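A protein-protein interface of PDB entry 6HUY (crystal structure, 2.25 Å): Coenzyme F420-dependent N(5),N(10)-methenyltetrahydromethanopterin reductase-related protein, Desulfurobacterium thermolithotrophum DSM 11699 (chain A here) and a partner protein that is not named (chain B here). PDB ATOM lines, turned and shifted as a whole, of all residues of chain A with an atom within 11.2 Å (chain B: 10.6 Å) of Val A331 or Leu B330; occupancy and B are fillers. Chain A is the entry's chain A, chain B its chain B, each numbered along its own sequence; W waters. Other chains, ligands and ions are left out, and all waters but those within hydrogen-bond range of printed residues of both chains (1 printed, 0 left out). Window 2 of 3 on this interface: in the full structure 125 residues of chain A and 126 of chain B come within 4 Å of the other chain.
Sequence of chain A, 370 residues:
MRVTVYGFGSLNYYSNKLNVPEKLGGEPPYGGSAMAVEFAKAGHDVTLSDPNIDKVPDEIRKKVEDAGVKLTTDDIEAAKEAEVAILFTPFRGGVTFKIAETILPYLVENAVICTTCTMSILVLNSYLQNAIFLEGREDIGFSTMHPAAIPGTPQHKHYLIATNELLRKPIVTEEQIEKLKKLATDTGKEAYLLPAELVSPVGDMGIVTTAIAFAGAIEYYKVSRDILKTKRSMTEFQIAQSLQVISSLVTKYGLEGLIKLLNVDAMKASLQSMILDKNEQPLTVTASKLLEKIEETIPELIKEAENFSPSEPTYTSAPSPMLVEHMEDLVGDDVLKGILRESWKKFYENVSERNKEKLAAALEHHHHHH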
ATOM      1  N   ARG A 168       7.562  17.074 -39.646  1.00  0.00           N
ATOM      2  CA  ARG A 168       6.463  16.203 -40.044  1.00  0.00           C
ATOM      3  C   ARG A 168       6.082  16.382 -41.503  1.00  0.00           C
ATOM      4  O   ARG A 168       5.485  15.480 -42.097  1.00  0.00           O
ATOM      5  CB  ARG A 168       5.230  16.551 -39.208  1.00  0.00           C
ATOM      6  CG  ARG A 168       4.723  15.531 -38.291  1.00  0.00           C
ATOM      7  CD  ARG A 168       3.982  16.242 -37.179  1.00  0.00           C
ATOM      8  NE  ARG A 168       4.922  16.631 -36.144  1.00  0.00           N
ATOM      9  CZ  ARG A 168       4.984  16.108 -34.928  1.00  0.00           C
ATOM     10  NH1 ARG A 168       5.908  16.555 -34.076  1.00  0.00           N
ATOM     11  NH2 ARG A 168       4.125  15.162 -34.562  1.00  0.00           N
ATOM     12  N   LEU A 323       3.989  17.905 -24.489  1.00  0.00           N
ATOM     13  CA  LEU A 323       2.929  18.849 -24.810  1.00  0.00           C
ATOM     14  C   LEU A 323       2.852  19.108 -26.306  1.00  0.00           C
ATOM     15  O   LEU A 323       1.752  19.292 -26.836  1.00  0.00           O
ATOM     16  CB  LEU A 323       3.140  20.169 -24.070  1.00  0.00           C
ATOM     17  CG  LEU A 323       3.221  20.124 -22.550  1.00  0.00           C
ATOM     18  CD1 LEU A 323       3.580  21.530 -22.015  1.00  0.00           C
ATOM     19  CD2 LEU A 323       1.950  19.632 -21.963  1.00  0.00           C
ATOM     20  N   VAL A 324       3.998  19.116 -27.000  1.00  0.00           N
ATOM     21  CA  VAL A 324       4.003  19.300 -28.449  1.00  0.00           C
ATOM     22  C   VAL A 324       3.133  18.244 -29.131  1.00  0.00           C
ATOM     23  O   VAL A 324       2.338  18.551 -30.029  1.00  0.00           O
ATOM     24  CB  VAL A 324       5.441  19.261 -28.992  1.00  0.00           C
ATOM     25  CG1 VAL A 324       5.442  18.995 -30.494  1.00  0.00           C
ATOM     26  CG2 VAL A 324       6.171  20.576 -28.677  1.00  0.00           C
ATOM     27  N   GLU A 325       3.292  16.978 -28.739  1.00  0.00           N
ATOM     28  CA  GLU A 325       2.532  15.926 -29.410  1.00  0.00           C
ATOM     29  C   GLU A 325       1.059  15.971 -29.030  1.00  0.00           C
ATOM     30  O   GLU A 325       0.204  15.674 -29.867  1.00  0.00           O
ATOM     31  CB  GLU A 325       3.150  14.560 -29.117  1.00  0.00           C
ATOM     32  CG  GLU A 325       4.562  14.351 -29.750  1.00  0.00           C
ATOM     33  CD  GLU A 325       4.676  14.861 -31.212  1.00  0.00           C
ATOM     34  OE1 GLU A 325       5.623  15.626 -31.520  1.00  0.00           O
ATOM     35  OE2 GLU A 325       3.821  14.485 -32.054  1.00  0.00           O
ATOM     36  N   HIS A 326       0.734  16.356 -27.790  1.00  0.00           N
ATOM     37  CA  HIS A 326      -0.668  16.580 -27.436  1.00  0.00           C
ATOM     38  C   HIS A 326      -1.283  17.699 -28.280  1.00  0.00           C
ATOM     39  O   HIS A 326      -2.437  17.600 -28.721  1.00  0.00           O
ATOM     40  CB  HIS A 326      -0.789  16.926 -25.951  1.00  0.00           C
ATOM     41  CG  HIS A 326      -0.665  15.744 -25.037  1.00  0.00           C
ATOM     42  ND1 HIS A 326      -1.612  14.747 -24.979  1.00  0.00           N
ATOM     43  CD2 HIS A 326       0.297  15.404 -24.145  1.00  0.00           C
ATOM     44  CE1 HIS A 326      -1.238  13.841 -24.092  1.00  0.00           C
ATOM     45  NE2 HIS A 326      -0.083  14.216 -23.574  1.00  0.00           N
ATOM     46  N   MET A 327      -0.527  18.779 -28.510  1.00  0.00           N
ATOM     47  CA  MET A 327      -1.017  19.876 -29.338  1.00  0.00           C
ATOM     48  C   MET A 327      -1.163  19.449 -30.788  1.00  0.00           C
ATOM     49  O   MET A 327      -2.131  19.829 -31.460  1.00  0.00           O
ATOM     50  CB  MET A 327      -0.069  21.065 -29.241  1.00  0.00           C
ATOM     51  CG  MET A 327      -0.362  22.008 -28.130  1.00  0.00           C
ATOM     52  SD  MET A 327      -1.719  23.088 -28.579  1.00  0.00           S
ATOM     53  CE  MET A 327      -0.846  24.103 -29.736  1.00  0.00           C
ATOM     54  N   GLU A 328      -0.185  18.697 -31.297  1.00  0.00           N
ATOM     55  CA  GLU A 328      -0.249  18.201 -32.661  1.00  0.00           C
ATOM     56  C   GLU A 328      -1.544  17.434 -32.881  1.00  0.00           C
ATOM     57  O   GLU A 328      -2.245  17.654 -33.870  1.00  0.00           O
ATOM     58  CB  GLU A 328       0.962  17.304 -32.959  1.00  0.00           C
ATOM     59  CG  GLU A 328       2.264  18.028 -33.219  1.00  0.00           C
ATOM     60  CD  GLU A 328       2.393  18.528 -34.649  1.00  0.00           C
ATOM     61  OE1 GLU A 328       1.449  18.323 -35.450  1.00  0.00           O
ATOM     62  OE2 GLU A 328       3.457  19.114 -34.991  1.00  0.00           O
ATOM     63  N   ASP A 329      -1.893  16.551 -31.936  1.00  0.00           N
ATOM     64  CA  ASP A 329      -3.084  15.721 -32.071  1.00  0.00           C
ATOM     65  C   ASP A 329      -4.356  16.550 -32.037  1.00  0.00           C
ATOM     66  O   ASP A 329      -5.329  16.208 -32.706  1.00  0.00           O
ATOM     67  CB  ASP A 329      -3.098  14.659 -30.961  1.00  0.00           C
ATOM     68  CG  ASP A 329      -3.680  13.319 -31.427  1.00  0.00           C
ATOM     69  OD1 ASP A 329      -3.731  13.049 -32.649  1.00  0.00           O
ATOM     70  OD2 ASP A 329      -4.113  12.529 -30.562  1.00  0.00           O
ATOM     71  N   LEU A 330      -4.372  17.645 -31.283  1.00  0.00           N
ATOM     72  CA  LEU A 330      -5.569  18.474 -31.177  1.00  0.00           C
ATOM     73  C   LEU A 330      -5.782  19.346 -32.412  1.00  0.00           C
ATOM     74  O   LEU A 330      -6.898  19.417 -32.943  1.00  0.00           O
ATOM     75  CB  LEU A 330      -5.483  19.365 -29.939  1.00  0.00           C
ATOM     76  CG  LEU A 330      -5.937  18.746 -28.627  1.00  0.00           C
ATOM     77  CD1 LEU A 330      -5.430  19.594 -27.461  1.00  0.00           C
ATOM     78  CD2 LEU A 330      -7.423  18.641 -28.604  1.00  0.00           C
ATOM     79  N   VAL A 331      -4.736  20.040 -32.874  1.00  0.00           N
ATOM     80  CA  VAL A 331      -4.900  21.133 -33.825  1.00  0.00           C
ATOM     81  C   VAL A 331      -3.914  21.091 -34.978  1.00  0.00           C
ATOM     82  O   VAL A 331      -3.984  21.950 -35.862  1.00  0.00           O
ATOM     83  CB  VAL A 331      -4.819  22.494 -33.110  1.00  0.00           C
ATOM     84  CG1 VAL A 331      -6.068  22.735 -32.288  1.00  0.00           C
ATOM     85  CG2 VAL A 331      -3.573  22.570 -32.228  1.00  0.00           C
ATOM     86  N   GLY A 332      -2.962  20.167 -34.984  1.00  0.00           N
ATOM     87  CA  GLY A 332      -2.157  19.936 -36.164  1.00  0.00           C
ATOM     88  C   GLY A 332      -0.848  20.717 -36.206  1.00  0.00           C
ATOM     89  O   GLY A 332      -0.562  21.595 -35.385  1.00  0.00           O
ATOM     90  N   ASP A 333      -0.062  20.398 -37.239  1.00  0.00           N
ATOM     91  CA  ASP A 333       1.327  20.842 -37.322  1.00  0.00           C
ATOM     92  C   ASP A 333       1.450  22.345 -37.574  1.00  0.00           C
ATOM     93  O   ASP A 333       2.352  22.997 -37.035  1.00  0.00           O
ATOM     94  CB  ASP A 333       2.039  20.073 -38.439  1.00  0.00           C
ATOM     95  CG  ASP A 333       3.541  20.233 -38.389  1.00  0.00           C
ATOM     96  OD1 ASP A 333       4.107  20.012 -37.307  1.00  0.00           O
ATOM     97  OD2 ASP A 333       4.158  20.590 -39.415  1.00  0.00           O
ATOM     98  N   ASP A 334       0.572  22.914 -38.398  1.00  0.00           N
ATOM     99  CA  ASP A 334       0.697  24.331 -38.714  1.00  0.00           C
ATOM    100  C   ASP A 334       0.585  25.199 -37.472  1.00  0.00           C
ATOM    101  O   ASP A 334       1.256  26.237 -37.382  1.00  0.00           O
ATOM    102  CB  ASP A 334      -0.357  24.728 -39.743  1.00  0.00           C
ATOM    103  CG  ASP A 334      -0.094  24.112 -41.087  1.00  0.00           C
ATOM    104  OD1 ASP A 334       1.072  23.762 -41.364  1.00  0.00           O
ATOM    105  OD2 ASP A 334      -1.053  23.946 -41.862  1.00  0.00           O
ATOM    106  N   VAL A 335      -0.241  24.793 -36.498  1.00  0.00           N
ATOM    107  CA  VAL A 335      -0.351  25.572 -35.266  1.00  0.00           C
ATOM    108  C   VAL A 335       0.955  25.522 -34.480  1.00  0.00           C
ATOM    109  O   VAL A 335       1.354  26.517 -33.859  1.00  0.00           O
ATOM    110  CB  VAL A 335      -1.537  25.098 -34.407  1.00  0.00           C
ATOM    111  CG1 VAL A 335      -1.520  25.799 -33.032  1.00  0.00           C
ATOM    112  CG2 VAL A 335      -2.856  25.362 -35.132  1.00  0.00           C
ATOM    113  N   LEU A 336       1.642  24.374 -34.475  1.00  0.00           N
ATOM    114  CA  LEU A 336       2.911  24.285 -33.743  1.00  0.00           C
ATOM    115  C   LEU A 336       3.970  25.199 -34.348  1.00  0.00           C
ATOM    116  O   LEU A 336       4.672  25.913 -33.621  1.00  0.00           O
ATOM    117  CB  LEU A 336       3.415  22.838 -33.713  1.00  0.00           C
ATOM    118  CG  LEU A 336       2.911  21.955 -32.579  1.00  0.00           C
ATOM    119  CD1 LEU A 336       3.407  22.461 -31.238  1.00  0.00           C
ATOM    120  CD2 LEU A 336       1.404  21.890 -32.608  1.00  0.00           C
ATOM    121  N   LYS A 337       4.091  25.204 -35.678  1.00  0.00           N
ATOM    122  CA  LYS A 337       5.001  26.133 -36.333  1.00  0.00           C
ATOM    123  C   LYS A 337       4.575  27.572 -36.058  1.00  0.00           C
ATOM    124  O   LYS A 337       5.420  28.472 -35.924  1.00  0.00           O
ATOM    125  CB  LYS A 337       5.032  25.862 -37.839  1.00  0.00           C
ATOM    126  CG  LYS A 337       5.447  24.434 -38.249  1.00  0.00           C
ATOM    127  CD  LYS A 337       6.254  24.415 -39.552  1.00  0.00           C
ATOM    128  CE  LYS A 337       5.378  24.713 -40.765  1.00  0.00           C
ATOM    129  NZ  LYS A 337       5.858  24.066 -42.029  1.00  0.00           N
ATOM    130  N   GLY A 338       3.257  27.811 -35.989  1.00  0.00           N
ATOM    131  CA  GLY A 338       2.763  29.126 -35.618  1.00  0.00           C
ATOM    132  C   GLY A 338       3.210  29.543 -34.234  1.00  0.00           C
ATOM    133  O   GLY A 338       3.469  30.727 -33.987  1.00  0.00           O
ATOM    134  N   ILE A 339       3.333  28.578 -33.317  1.00  0.00           N
ATOM    135  CA  ILE A 339       3.819  28.885 -31.978  1.00  0.00           C
ATOM    136  C   ILE A 339       5.289  29.288 -32.023  1.00  0.00           C
ATOM    137  O   ILE A 339       5.698  30.258 -31.374  1.00  0.00           O
ATOM    138  CB  ILE A 339       3.563  27.683 -31.050  1.00  0.00           C
ATOM    139  CG1 ILE A 339       2.108  27.689 -30.604  1.00  0.00           C
ATOM    140  CG2 ILE A 339       4.459  27.696 -29.845  1.00  0.00           C
ATOM    141  CD1 ILE A 339       1.582  26.336 -30.298  1.00  0.00           C
ATOM    142  N   GLU A 342       5.162  32.771 -33.190  1.00  0.00           N
ATOM    143  CA  GLU A 342       4.713  33.654 -32.120  1.00  0.00           C
ATOM    144  C   GLU A 342       5.818  33.867 -31.086  1.00  0.00           C
ATOM    145  O   GLU A 342       5.996  34.979 -30.577  1.00  0.00           O
ATOM    146  CB  GLU A 342       3.448  33.073 -31.478  1.00  0.00           C
ATOM    147  CG  GLU A 342       2.886  33.858 -30.288  1.00  0.00           C
ATOM    148  CD  GLU A 342       1.741  33.125 -29.580  1.00  0.00           C
ATOM    149  OE1 GLU A 342       1.409  31.984 -29.988  1.00  0.00           O
ATOM    150  OE2 GLU A 342       1.166  33.696 -28.624  1.00  0.00           O
ATOM    151  N   TYR B 315       9.194  18.989 -32.067  1.00  0.00           N
ATOM    152  CA  TYR B 315       9.691  20.353 -31.981  1.00  0.00           C
ATOM    153  C   TYR B 315      10.428  20.466 -30.661  1.00  0.00           C
ATOM    154  O   TYR B 315       9.902  20.083 -29.612  1.00  0.00           O
ATOM    155  CB  TYR B 315       8.564  21.383 -32.104  1.00  0.00           C
ATOM    156  CG  TYR B 315       8.008  21.455 -33.516  1.00  0.00           C
ATOM    157  CD1 TYR B 315       8.752  22.037 -34.555  1.00  0.00           C
ATOM    158  CD2 TYR B 315       6.751  20.925 -33.816  1.00  0.00           C
ATOM    159  CE1 TYR B 315       8.264  22.079 -35.834  1.00  0.00           C
ATOM    160  CE2 TYR B 315       6.253  20.973 -35.085  1.00  0.00           C
ATOM    161  CZ  TYR B 315       7.010  21.542 -36.093  1.00  0.00           C
ATOM    162  OH  TYR B 315       6.511  21.581 -37.360  1.00  0.00           O
ATOM    163  N   MET B 322       4.107  28.598 -23.380  1.00  0.00           N
ATOM    164  CA  MET B 322       3.234  28.888 -24.511  1.00  0.00           C
ATOM    165  C   MET B 322       2.345  27.692 -24.848  1.00  0.00           C
ATOM    166  O   MET B 322       1.165  27.863 -25.180  1.00  0.00           O
ATOM    167  CB  MET B 322       4.065  29.295 -25.719  1.00  0.00           C
ATOM    168  CG  MET B 322       4.710  30.669 -25.578  1.00  0.00           C
ATOM    169  SD  MET B 322       5.567  31.198 -27.066  1.00  0.00           S
ATOM    170  CE  MET B 322       4.189  31.303 -28.193  1.00  0.00           C
ATOM    171  N   LEU B 323       2.892  26.478 -24.776  1.00  0.00           N
ATOM    172  CA  LEU B 323       2.090  25.294 -25.063  1.00  0.00           C
ATOM    173  C   LEU B 323       0.987  25.135 -24.037  1.00  0.00           C
ATOM    174  O   LEU B 323      -0.154  24.816 -24.390  1.00  0.00           O
ATOM    175  CB  LEU B 323       2.975  24.049 -25.104  1.00  0.00           C
ATOM    176  CG  LEU B 323       3.989  23.983 -26.244  1.00  0.00           C
ATOM    177  CD1 LEU B 323       4.979  22.859 -26.011  1.00  0.00           C
ATOM    178  CD2 LEU B 323       3.295  23.784 -27.607  1.00  0.00           C
ATOM    179  N   VAL B 324       1.297  25.388 -22.761  1.00  0.00           N
ATOM    180  CA  VAL B 324       0.280  25.303 -21.718  1.00  0.00           C
ATOM    181  C   VAL B 324      -0.809  26.345 -21.948  1.00  0.00           C
ATOM    182  O   VAL B 324      -2.005  26.043 -21.847  1.00  0.00           O
ATOM    183  CB  VAL B 324       0.919  25.443 -20.323  1.00  0.00           C
ATOM    184  CG1 VAL B 324      -0.145  25.476 -19.229  1.00  0.00           C
ATOM    185  CG2 VAL B 324       1.857  24.303 -20.088  1.00  0.00           C
ATOM    186  N   GLU B 325      -0.417  27.580 -22.289  1.00  0.00           N
ATOM    187  CA  GLU B 325      -1.402  28.639 -22.501  1.00  0.00           C
ATOM    188  C   GLU B 325      -2.316  28.317 -23.673  1.00  0.00           C
ATOM    189  O   GLU B 325      -3.536  28.489 -23.586  1.00  0.00           O
ATOM    190  CB  GLU B 325      -0.705  29.979 -22.727  1.00  0.00           C
ATOM    191  CG  GLU B 325      -0.252  30.631 -21.449  1.00  0.00           C
ATOM    192  CD  GLU B 325       0.491  31.937 -21.674  1.00  0.00           C
ATOM    193  OE1 GLU B 325       0.052  32.741 -22.531  1.00  0.00           O
ATOM    194  OE2 GLU B 325       1.516  32.148 -20.977  1.00  0.00           O
ATOM    195  N   HIS B 326      -1.739  27.874 -24.792  1.00  0.00           N
ATOM    196  CA  HIS B 326      -2.555  27.517 -25.948  1.00  0.00           C
ATOM    197  C   HIS B 326      -3.515  26.386 -25.609  1.00  0.00           C
ATOM    198  O   HIS B 326      -4.675  26.391 -26.034  1.00  0.00           O
ATOM    199  CB  HIS B 326      -1.666  27.109 -27.121  1.00  0.00           C
ATOM    200  CG  HIS B 326      -1.274  28.242 -28.013  1.00  0.00           C
ATOM    201  ND1 HIS B 326      -1.822  28.422 -29.267  1.00  0.00           N
ATOM    202  CD2 HIS B 326      -0.379  29.245 -27.846  1.00  0.00           C
ATOM    203  CE1 HIS B 326      -1.289  29.494 -29.829  1.00  0.00           C
ATOM    204  NE2 HIS B 326      -0.411  30.013 -28.986  1.00  0.00           N
ATOM    205  N   MET B 327      -3.039  25.407 -24.843  1.00  0.00           N
ATOM    206  CA  MET B 327      -3.869  24.277 -24.462  1.00  0.00           C
ATOM    207  C   MET B 327      -5.014  24.696 -23.545  1.00  0.00           C
ATOM    208  O   MET B 327      -6.095  24.093 -23.591  1.00  0.00           O
ATOM    209  CB  MET B 327      -2.998  23.233 -23.789  1.00  0.00           C
ATOM    210  CG  MET B 327      -3.406  21.831 -24.109  1.00  0.00           C
ATOM    211  SD  MET B 327      -2.227  21.030 -25.194  1.00  0.00           S
ATOM    212  CE  MET B 327      -0.873  20.927 -24.034  1.00  0.00           C
ATOM    213  N   GLU B 328      -4.803  25.725 -22.716  1.00  0.00           N
ATOM    214  CA  GLU B 328      -5.871  26.215 -21.847  1.00  0.00           C
ATOM    215  C   GLU B 328      -7.040  26.748 -22.657  1.00  0.00           C
ATOM    216  O   GLU B 328      -8.190  26.653 -22.221  1.00  0.00           O
ATOM    217  CB  GLU B 328      -5.363  27.319 -20.920  1.00  0.00           C
ATOM    218  CG  GLU B 328      -4.637  26.849 -19.686  1.00  0.00           C
ATOM    219  CD  GLU B 328      -4.076  28.016 -18.876  1.00  0.00           C
ATOM    220  OE1 GLU B 328      -4.162  29.166 -19.367  1.00  0.00           O
ATOM    221  OE2 GLU B 328      -3.554  27.784 -17.757  1.00  0.00           O
ATOM    222  N   ASP B 329      -6.764  27.337 -23.822  1.00  0.00           N
ATOM    223  CA  ASP B 329      -7.820  27.884 -24.666  1.00  0.00           C
ATOM    224  C   ASP B 329      -8.464  26.820 -25.546  1.00  0.00           C
ATOM    225  O   ASP B 329      -9.573  27.032 -26.046  1.00  0.00           O
ATOM    226  CB  ASP B 329      -7.269  29.011 -25.548  1.00  0.00           C
ATOM    227  CG  ASP B 329      -6.684  30.165 -24.738  1.00  0.00           C
ATOM    228  OD1 ASP B 329      -7.256  30.501 -23.672  1.00  0.00           O
ATOM    229  OD2 ASP B 329      -5.652  30.733 -25.174  1.00  0.00           O
ATOM    230  N   LEU B 330      -7.791  25.688 -25.764  1.00  0.00           N
ATOM    231  CA  LEU B 330      -8.350  24.649 -26.625  1.00  0.00           C
ATOM    232  C   LEU B 330      -9.220  23.671 -25.850  1.00  0.00           C
ATOM    233  O   LEU B 330     -10.239  23.207 -26.367  1.00  0.00           O
ATOM    234  CB  LEU B 330      -7.224  23.890 -27.338  1.00  0.00           C
ATOM    235  CG  LEU B 330      -6.391  24.675 -28.359  1.00  0.00           C
ATOM    236  CD1 LEU B 330      -5.263  23.807 -28.902  1.00  0.00           C
ATOM    237  CD2 LEU B 330      -7.251  25.210 -29.488  1.00  0.00           C
ATOM    238  N   VAL B 331      -8.855  23.352 -24.610  1.00  0.00           N
ATOM    239  CA  VAL B 331      -9.568  22.336 -23.848  1.00  0.00           C
ATOM    240  C   VAL B 331      -9.866  22.866 -22.454  1.00  0.00           C
ATOM    241  O   VAL B 331      -9.266  23.836 -21.991  1.00  0.00           O
ATOM    242  CB  VAL B 331      -8.777  21.004 -23.784  1.00  0.00           C
ATOM    243  CG1 VAL B 331      -8.261  20.634 -25.163  1.00  0.00           C
ATOM    244  CG2 VAL B 331      -7.602  21.074 -22.819  1.00  0.00           C
ATOM    245  N   GLY B 332     -10.810  22.226 -21.784  1.00  0.00           N
ATOM    246  CA  GLY B 332     -11.131  22.634 -20.431  1.00  0.00           C
ATOM    247  C   GLY B 332      -9.956  22.463 -19.482  1.00  0.00           C
ATOM    248  O   GLY B 332      -9.033  21.681 -19.720  1.00  0.00           O
ATOM    249  N   ASP B 333      -9.976  23.235 -18.385  1.00  0.00           N
ATOM    250  CA  ASP B 333      -8.911  23.103 -17.392  1.00  0.00           C
ATOM    251  C   ASP B 333      -8.921  21.709 -16.785  1.00  0.00           C
ATOM    252  O   ASP B 333      -7.864  21.152 -16.465  1.00  0.00           O
ATOM    253  CB  ASP B 333      -9.050  24.166 -16.297  1.00  0.00           C
ATOM    254  CG  ASP B 333      -7.792  24.281 -15.429  1.00  0.00           C
ATOM    255  OD1 ASP B 333      -7.155  23.246 -15.132  1.00  0.00           O
ATOM    256  OD2 ASP B 333      -7.425  25.413 -15.049  1.00  0.00           O
ATOM    257  N   ASP B 334     -10.104  21.122 -16.655  1.00  0.00           N
ATOM    258  CA  ASP B 334     -10.203  19.754 -16.168  1.00  0.00           C
ATOM    259  C   ASP B 334      -9.448  18.784 -17.081  1.00  0.00           C
ATOM    260  O   ASP B 334      -8.747  17.882 -16.606  1.00  0.00           O
ATOM    261  CB  ASP B 334     -11.677  19.386 -16.046  1.00  0.00           C
ATOM    262  CG  ASP B 334     -11.936  18.407 -14.928  1.00  0.00           C
ATOM    263  OD1 ASP B 334     -10.974  17.720 -14.522  1.00  0.00           O
ATOM    264  OD2 ASP B 334     -13.095  18.328 -14.455  1.00  0.00           O
ATOM    265  N   VAL B 335      -9.554  18.980 -18.397  1.00  0.00           N
ATOM    266  CA  VAL B 335      -8.853  18.124 -19.350  1.00  0.00           C
ATOM    267  C   VAL B 335      -7.358  18.417 -19.341  1.00  0.00           C
ATOM    268  O   VAL B 335      -6.530  17.506 -19.456  1.00  0.00           O
ATOM    269  CB  VAL B 335      -9.466  18.314 -20.749  1.00  0.00           C
ATOM    270  CG1 VAL B 335      -8.641  17.607 -21.809  1.00  0.00           C
ATOM    271  CG2 VAL B 335     -10.915  17.820 -20.745  1.00  0.00           C
ATOM    272  N   LEU B 336      -6.989  19.694 -19.214  1.00  0.00           N
ATOM    273  CA  LEU B 336      -5.584  20.080 -19.199  1.00  0.00           C
ATOM    274  C   LEU B 336      -4.828  19.429 -18.041  1.00  0.00           C
ATOM    275  O   LEU B 336      -3.682  18.995 -18.212  1.00  0.00           O
ATOM    276  CB  LEU B 336      -5.477  21.605 -19.128  1.00  0.00           C
ATOM    277  CG  LEU B 336      -4.070  22.221 -19.077  1.00  0.00           C
ATOM    278  CD1 LEU B 336      -3.200  21.794 -20.278  1.00  0.00           C
ATOM    279  CD2 LEU B 336      -4.173  23.739 -18.993  1.00  0.00           C
ATOM    280  N   ILE B 339      -3.836  16.068 -19.020  1.00  0.00           N
ATOM    281  CA  ILE B 339      -2.778  16.056 -20.027  1.00  0.00           C
ATOM    282  C   ILE B 339      -1.421  16.345 -19.383  1.00  0.00           C
ATOM    283  O   ILE B 339      -0.419  15.679 -19.679  1.00  0.00           O
ATOM    284  CB  ILE B 339      -3.114  17.058 -21.153  1.00  0.00           C
ATOM    285  CG1 ILE B 339      -4.215  16.478 -22.050  1.00  0.00           C
ATOM    286  CG2 ILE B 339      -1.885  17.413 -21.982  1.00  0.00           C
ATOM    287  CD1 ILE B 339      -4.903  17.527 -22.911  1.00  0.00           C
HETATM  288  O   HOH W   1       6.644  19.844 -39.708  1.00  0.00           O
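Water W1 lies within hydrogen-bond range of the side-chain carboxylate (OD2) of Asp A333 (2.6 Å), the backbone NH (N) of Arg A168 (2.9 Å) and the side-chain hydroxyl (OH) of Tyr B315 (2.9 Å).
Among the printed residues, pairs that only touch across the chains: Lys A337 with Tyr B315, Glu A342 with Met B322, Glu A328 with Tyr B315, Met A327 with Met B327, Met A327 with Leu B330, Val A331 with Leu B330, Leu A336 with Tyr B315, His A326 with Ile B339, Ile A339 with Met B322, Val A324 with Leu B323, Leu A323 with Met B327, Ile A339 with His B326, Leu A323 with Val B324, Leu A330 with Val B331, Leu A323 with Leu B323, Leu A336 with Leu B323 and Val A324 with Tyr B315.
Of the printed residues of chain B, Val A331 touches Leu B330. Leu B330 touches two residues of chain A. Met A327 touches two residues of chain B. Leu A330 touches just one residue of chain B: Val B331. No residue of chain B comes within 4 Å of Gly A332. No residue of chain B comes within 4 Å of Val A335. Asp B329 touches none of the printed residues of chain A. Val B331 touches just one residue of chain A: Leu A330. Printed residues of chain A within 4 Å of Leu B323: Leu A323, Val A324 and Leu A336. Printed residues of chain A within 4 Å of Tyr B315: Val A324, Glu A328, Asp A333, Leu A336 and Lys A337. Printed residues of chain A within 4 Å of Ile B339: His A326 (3.7 Å). Asp B334 touches none of the printed residues of chain A. The nearest printed residue of chain A that does not touch Tyr B315 is Arg A168 (4.5 Å).
The side-chain carboxylate (OD1) of Asp A333 lies within hydrogen-bond range of the side-chain hydroxyl (OH) of Tyr B315 (2.9 Å). The side-chain carboxylate (OE1) of Glu A342 is in hydrogen-bond range of a ring nitrogen (NE2) of His B326 (2.9 Å).
Hydrophobic or aromatic side chains of chain B that line the printed part of chain A: Tyr B315, Met B322, Leu B323, Val B324, His B326, Met B327, Leu B330, Val B331 and Ile B339. Of the 19 printed residues of chain A, 12 touch a printed residue of chain B. Hydrophobic or aromatic side chains of chain A that line the printed part of chain B: Leu A323, Val A324, His A326, Met A327, Leu A330, Val A331, Leu A336 and Ile A339. Among the printed residues, no Asp or Glu carboxylate lies within 4 Å of a Lys or Arg side-chain nitrogen of the other chain.
OE2 of Glu A328 lies within salt-bridge range of NE of Arg A168 (3.1 Å). OD1 of Asp A333 lies within salt-bridge range of NE of Arg A168 (3.7 Å). The side-chain carboxylate (OE1) of Glu A328 lies within hydrogen-bond range of the backbone NH (N) of Asp A333 (3.1 Å).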
